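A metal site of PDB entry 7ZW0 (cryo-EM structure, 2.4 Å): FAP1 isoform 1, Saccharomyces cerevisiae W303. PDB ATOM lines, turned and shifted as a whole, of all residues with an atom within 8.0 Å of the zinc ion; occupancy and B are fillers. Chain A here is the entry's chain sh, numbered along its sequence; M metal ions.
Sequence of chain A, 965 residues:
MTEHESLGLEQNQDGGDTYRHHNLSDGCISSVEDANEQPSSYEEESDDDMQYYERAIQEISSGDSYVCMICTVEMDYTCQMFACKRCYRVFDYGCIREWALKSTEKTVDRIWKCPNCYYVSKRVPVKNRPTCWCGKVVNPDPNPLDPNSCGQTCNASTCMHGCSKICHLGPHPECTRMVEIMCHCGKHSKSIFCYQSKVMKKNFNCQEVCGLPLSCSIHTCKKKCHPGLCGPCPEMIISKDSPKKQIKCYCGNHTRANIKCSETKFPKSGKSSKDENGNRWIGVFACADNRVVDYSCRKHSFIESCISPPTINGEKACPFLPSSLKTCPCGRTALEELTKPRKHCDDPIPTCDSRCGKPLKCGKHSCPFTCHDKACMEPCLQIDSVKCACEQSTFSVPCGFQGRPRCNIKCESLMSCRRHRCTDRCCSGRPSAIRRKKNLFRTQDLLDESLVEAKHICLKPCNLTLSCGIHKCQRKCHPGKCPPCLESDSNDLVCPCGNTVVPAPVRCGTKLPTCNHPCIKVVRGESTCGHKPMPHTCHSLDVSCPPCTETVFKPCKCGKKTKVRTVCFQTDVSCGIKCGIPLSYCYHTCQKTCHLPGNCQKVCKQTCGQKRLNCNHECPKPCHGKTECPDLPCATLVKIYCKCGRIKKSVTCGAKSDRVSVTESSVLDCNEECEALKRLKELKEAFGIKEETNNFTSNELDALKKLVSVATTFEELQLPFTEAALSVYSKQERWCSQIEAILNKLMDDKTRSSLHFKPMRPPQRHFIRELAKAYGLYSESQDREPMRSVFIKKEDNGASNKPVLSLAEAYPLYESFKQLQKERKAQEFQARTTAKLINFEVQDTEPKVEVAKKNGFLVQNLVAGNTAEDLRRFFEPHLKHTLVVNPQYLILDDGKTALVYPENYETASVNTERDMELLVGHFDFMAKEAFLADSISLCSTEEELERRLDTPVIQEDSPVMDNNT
The backbone NH (N) of Cys 473 sits at hydrogen-bond distance from the backbone carbonyl oxygen (O) of Leu 464, at 2.8 Å. The side-chain sulfur (SG) of Cys 473 lies close to the backbone NH (N) of Arg 475, 3.6 Å away. N of Cys 462 lies within hydrogen-bond range of O of Arg 475.
The nearest printed residue that does not touch the zinc ion is Pro 483 (4.2 Å).
The zinc ion is bound by SG of Cys 482, NE2 of His 478, SG of Cys 473 and SG of Cys 462. The zinc ion has four donor atoms within binding distance.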
ATOM      1  N   ARG A 419      -2.570  -1.609  15.303  1.00  0.00           N
ATOM      2  CA  ARG A 419      -2.151  -0.409  14.597  1.00  0.00           C
ATOM      3  C   ARG A 419      -0.660  -0.216  14.761  1.00  0.00           C
ATOM      4  O   ARG A 419      -0.077   0.676  14.133  1.00  0.00           O
ATOM      5  CB  ARG A 419      -2.893   0.807  15.150  1.00  0.00           C
ATOM      6  CG  ARG A 419      -4.407   0.641  15.200  1.00  0.00           C
ATOM      7  CD  ARG A 419      -5.101   1.839  15.831  1.00  0.00           C
ATOM      8  NE  ARG A 419      -4.886   3.076  15.095  1.00  0.00           N
ATOM      9  CZ  ARG A 419      -4.115   4.079  15.494  1.00  0.00           C
ATOM     10  NH1 ARG A 419      -3.982   5.165  14.745  1.00  0.00           N
ATOM     11  NH2 ARG A 419      -3.487   3.999  16.659  1.00  0.00           N
ATOM     12  N   PRO A 461      -2.915   5.302  24.285  1.00  0.00           N
ATOM     13  CA  PRO A 461      -4.258   5.861  24.050  1.00  0.00           C
ATOM     14  C   PRO A 461      -4.656   5.791  22.580  1.00  0.00           C
ATOM     15  O   PRO A 461      -3.792   5.974  21.717  1.00  0.00           O
ATOM     16  CB  PRO A 461      -4.122   7.324  24.494  1.00  0.00           C
ATOM     17  CG  PRO A 461      -2.643   7.594  24.529  1.00  0.00           C
ATOM     18  CD  PRO A 461      -1.999   6.292  24.875  1.00  0.00           C
ATOM     19  N   CYS A 462      -5.932   5.541  22.281  1.00  0.00           N
ATOM     20  CA  CYS A 462      -6.349   5.352  20.896  1.00  0.00           C
ATOM     21  C   CYS A 462      -6.118   6.566  20.011  1.00  0.00           C
ATOM     22  O   CYS A 462      -5.673   6.424  18.867  1.00  0.00           O
ATOM     23  CB  CYS A 462      -7.817   4.934  20.829  1.00  0.00           C
ATOM     24  SG  CYS A 462      -8.322   4.157  19.280  1.00  0.00           S
ATOM     25  N   ASN A 463      -6.426   7.763  20.520  1.00  0.00           N
ATOM     26  CA  ASN A 463      -6.165   8.998  19.764  1.00  0.00           C
ATOM     27  C   ASN A 463      -6.780   8.995  18.367  1.00  0.00           C
ATOM     28  O   ASN A 463      -6.143   9.433  17.414  1.00  0.00           O
ATOM     29  CB  ASN A 463      -4.663   9.288  19.691  1.00  0.00           C
ATOM     30  CG  ASN A 463      -4.036   9.446  21.060  1.00  0.00           C
ATOM     31  OD1 ASN A 463      -4.722   9.704  22.043  1.00  0.00           O
ATOM     32  ND2 ASN A 463      -2.711   9.313  21.122  1.00  0.00           N
ATOM     33  N   LEU A 464      -8.010   8.511  18.262  1.00  0.00           N
ATOM     34  CA  LEU A 464      -8.673   8.459  16.954  1.00  0.00           C
ATOM     35  C   LEU A 464     -10.017   9.172  17.000  1.00  0.00           C
ATOM     36  O   LEU A 464     -10.685   9.169  18.027  1.00  0.00           O
ATOM     37  CB  LEU A 464      -8.864   7.016  16.499  1.00  0.00           C
ATOM     38  CG  LEU A 464      -7.700   6.344  15.771  1.00  0.00           C
ATOM     39  CD1 LEU A 464      -8.091   4.937  15.360  1.00  0.00           C
ATOM     40  CD2 LEU A 464      -7.319   7.182  14.551  1.00  0.00           C
ATOM     41  N   THR A 465     -10.407   9.768  15.890  1.00  0.00           N
ATOM     42  CA  THR A 465     -11.651  10.534  15.863  1.00  0.00           C
ATOM     43  C   THR A 465     -12.874   9.676  16.113  1.00  0.00           C
ATOM     44  O   THR A 465     -12.943   8.528  15.673  1.00  0.00           O
ATOM     45  CB  THR A 465     -11.835  11.284  14.531  1.00  0.00           C
ATOM     46  OG1 THR A 465     -11.728  10.349  13.443  1.00  0.00           O
ATOM     47  CG2 THR A 465     -10.777  12.362  14.374  1.00  0.00           C
ATOM     48  N   LEU A 466     -13.842  10.231  16.825  1.00  0.00           N
ATOM     49  CA  LEU A 466     -15.075   9.498  17.134  1.00  0.00           C
ATOM     50  C   LEU A 466     -16.065   9.598  15.983  1.00  0.00           C
ATOM     51  O   LEU A 466     -15.737  10.126  14.918  1.00  0.00           O
ATOM     52  CB  LEU A 466     -15.694  10.007  18.426  1.00  0.00           C
ATOM     53  CG  LEU A 466     -14.883   9.688  19.677  1.00  0.00           C
ATOM     54  CD1 LEU A 466     -15.562  10.226  20.928  1.00  0.00           C
ATOM     55  CD2 LEU A 466     -14.675   8.189  19.785  1.00  0.00           C
ATOM     56  N   LYS A 472     -11.871  13.034  20.304  1.00  0.00           N
ATOM     57  CA  LYS A 472     -10.874  11.973  20.234  1.00  0.00           C
ATOM     58  C   LYS A 472     -11.254  10.845  21.180  1.00  0.00           C
ATOM     59  O   LYS A 472     -11.770  11.095  22.261  1.00  0.00           O
ATOM     60  CB  LYS A 472      -9.481  12.498  20.586  1.00  0.00           C
ATOM     61  CG  LYS A 472      -8.801  13.226  19.441  1.00  0.00           C
ATOM     62  CD  LYS A 472      -8.595  12.291  18.268  1.00  0.00           C
ATOM     63  CE  LYS A 472      -7.798  12.947  17.146  1.00  0.00           C
ATOM     64  NZ  LYS A 472      -7.526  11.995  16.037  1.00  0.00           N
ATOM     65  N   CYS A 473     -11.010   9.604  20.762  1.00  0.00           N
ATOM     66  CA  CYS A 473     -11.415   8.468  21.579  1.00  0.00           C
ATOM     67  C   CYS A 473     -10.703   8.496  22.919  1.00  0.00           C
ATOM     68  O   CYS A 473      -9.487   8.667  22.981  1.00  0.00           O
ATOM     69  CB  CYS A 473     -11.100   7.167  20.851  1.00  0.00           C
ATOM     70  SG  CYS A 473     -11.878   5.700  21.543  1.00  0.00           S
ATOM     71  N   GLN A 474     -11.461   8.322  24.003  1.00  0.00           N
ATOM     72  CA  GLN A 474     -10.872   8.335  25.336  1.00  0.00           C
ATOM     73  C   GLN A 474     -10.344   6.962  25.702  1.00  0.00           C
ATOM     74  O   GLN A 474      -9.589   6.818  26.660  1.00  0.00           O
ATOM     75  CB  GLN A 474     -11.921   8.772  26.356  1.00  0.00           C
ATOM     76  CG  GLN A 474     -12.678  10.032  25.956  1.00  0.00           C
ATOM     77  CD  GLN A 474     -13.867  10.301  26.840  1.00  0.00           C
ATOM     78  OE1 GLN A 474     -14.132   9.568  27.799  1.00  0.00           O
ATOM     79  NE2 GLN A 474     -14.613  11.355  26.540  1.00  0.00           N
ATOM     80  N   ARG A 475     -10.727   5.955  24.926  1.00  0.00           N
ATOM     81  CA  ARG A 475     -10.289   4.592  25.204  1.00  0.00           C
ATOM     82  C   ARG A 475      -8.843   4.356  24.842  1.00  0.00           C
ATOM     83  O   ARG A 475      -8.269   5.106  24.053  1.00  0.00           O
ATOM     84  CB  ARG A 475     -11.145   3.585  24.443  1.00  0.00           C
ATOM     85  CG  ARG A 475     -12.596   3.507  24.883  1.00  0.00           C
ATOM     86  CD  ARG A 475     -13.314   2.450  24.069  1.00  0.00           C
ATOM     87  NE  ARG A 475     -12.636   1.161  24.151  1.00  0.00           N
ATOM     88  CZ  ARG A 475     -12.961   0.096  23.432  1.00  0.00           C
ATOM     89  NH1 ARG A 475     -13.959   0.165  22.564  1.00  0.00           N
ATOM     90  NH2 ARG A 475     -12.284  -1.041  23.572  1.00  0.00           N
ATOM     91  N   LYS A 476      -8.237   3.335  25.420  1.00  0.00           N
ATOM     92  CA  LYS A 476      -6.875   2.972  25.050  1.00  0.00           C
ATOM     93  C   LYS A 476      -6.951   2.318  23.680  1.00  0.00           C
ATOM     94  O   LYS A 476      -8.040   1.936  23.234  1.00  0.00           O
ATOM     95  CB  LYS A 476      -6.241   2.037  26.068  1.00  0.00           C
ATOM     96  CG  LYS A 476      -6.885   0.662  26.138  1.00  0.00           C
ATOM     97  CD  LYS A 476      -5.832  -0.419  26.080  1.00  0.00           C
ATOM     98  CE  LYS A 476      -6.460  -1.789  25.854  1.00  0.00           C
ATOM     99  NZ  LYS A 476      -5.421  -2.815  25.589  1.00  0.00           N
ATOM    100  N   CYS A 477      -5.823   2.173  23.002  1.00  0.00           N
ATOM    101  CA  CYS A 477      -5.849   1.636  21.646  1.00  0.00           C
ATOM    102  C   CYS A 477      -6.534   0.290  21.605  1.00  0.00           C
ATOM    103  O   CYS A 477      -6.228  -0.603  22.394  1.00  0.00           O
ATOM    104  CB  CYS A 477      -4.426   1.490  21.111  1.00  0.00           C
ATOM    105  SG  CYS A 477      -3.749   2.970  20.324  1.00  0.00           S
ATOM    106  N   HIS A 478      -7.459   0.136  20.663  1.00  0.00           N
ATOM    107  CA  HIS A 478      -8.224  -1.099  20.575  1.00  0.00           C
ATOM    108  C   HIS A 478      -8.451  -1.495  19.133  1.00  0.00           C
ATOM    109  O   HIS A 478      -8.507  -0.642  18.248  1.00  0.00           O
ATOM    110  CB  HIS A 478      -9.571  -0.918  21.285  1.00  0.00           C
ATOM    111  CG  HIS A 478     -10.392   0.214  20.750  1.00  0.00           C
ATOM    112  ND1 HIS A 478     -11.299   0.044  19.729  1.00  0.00           N
ATOM    113  CD2 HIS A 478     -10.453   1.514  21.095  1.00  0.00           C
ATOM    114  CE1 HIS A 478     -11.884   1.205  19.459  1.00  0.00           C
ATOM    115  NE2 HIS A 478     -11.380   2.116  20.277  1.00  0.00           N
ATOM    116  N   PRO A 479      -8.584  -2.805  18.880  1.00  0.00           N
ATOM    117  CA  PRO A 479      -8.898  -3.236  17.514  1.00  0.00           C
ATOM    118  C   PRO A 479     -10.337  -2.877  17.140  1.00  0.00           C
ATOM    119  O   PRO A 479     -11.204  -2.818  18.006  1.00  0.00           O
ATOM    120  CB  PRO A 479      -8.728  -4.760  17.572  1.00  0.00           C
ATOM    121  CG  PRO A 479      -8.844  -5.112  19.021  1.00  0.00           C
ATOM    122  CD  PRO A 479      -8.311  -3.941  19.775  1.00  0.00           C
ATOM    123  N   GLY A 480     -10.575  -2.619  15.863  1.00  0.00           N
ATOM    124  CA  GLY A 480     -11.917  -2.282  15.408  1.00  0.00           C
ATOM    125  C   GLY A 480     -12.273  -0.816  15.457  1.00  0.00           C
ATOM    126  O   GLY A 480     -11.462   0.006  15.884  1.00  0.00           O
ATOM    127  N   LYS A 481     -13.483  -0.475  15.029  1.00  0.00           N
ATOM    128  CA  LYS A 481     -13.908   0.924  14.984  1.00  0.00           C
ATOM    129  C   LYS A 481     -14.134   1.583  16.336  1.00  0.00           C
ATOM    130  O   LYS A 481     -14.534   0.915  17.298  1.00  0.00           O
ATOM    131  CB  LYS A 481     -15.160   1.072  14.119  1.00  0.00           C
ATOM    132  CG  LYS A 481     -14.931   0.764  12.645  1.00  0.00           C
ATOM    133  CD  LYS A 481     -16.190   1.035  11.831  1.00  0.00           C
ATOM    134  CE  LYS A 481     -15.955   0.762  10.354  1.00  0.00           C
ATOM    135  NZ  LYS A 481     -17.168   1.040   9.541  1.00  0.00           N
ATOM    136  N   CYS A 482     -13.890   2.881  16.409  1.00  0.00           N
ATOM    137  CA  CYS A 482     -14.108   3.619  17.642  1.00  0.00           C
ATOM    138  C   CYS A 482     -15.586   3.722  17.992  1.00  0.00           C
ATOM    139  O   CYS A 482     -16.434   3.781  17.104  1.00  0.00           O
ATOM    140  CB  CYS A 482     -13.505   5.023  17.543  1.00  0.00           C
ATOM    141  SG  CYS A 482     -11.705   5.030  17.490  1.00  0.00           S
ATOM    142  N   PRO A 483     -15.905   3.737  19.292  1.00  0.00           N
ATOM    143  CA  PRO A 483     -17.297   3.834  19.738  1.00  0.00           C
ATOM    144  C   PRO A 483     -17.945   5.160  19.397  1.00  0.00           C
ATOM    145  O   PRO A 483     -17.250   6.168  19.262  1.00  0.00           O
ATOM    146  CB  PRO A 483     -17.192   3.680  21.268  1.00  0.00           C
ATOM    147  CG  PRO A 483     -15.902   2.967  21.484  1.00  0.00           C
ATOM    148  CD  PRO A 483     -14.992   3.484  20.422  1.00  0.00           C
HETATM  149 ZN    ZN M   1     -10.922   4.395  19.635  1.00  0.00          ZN
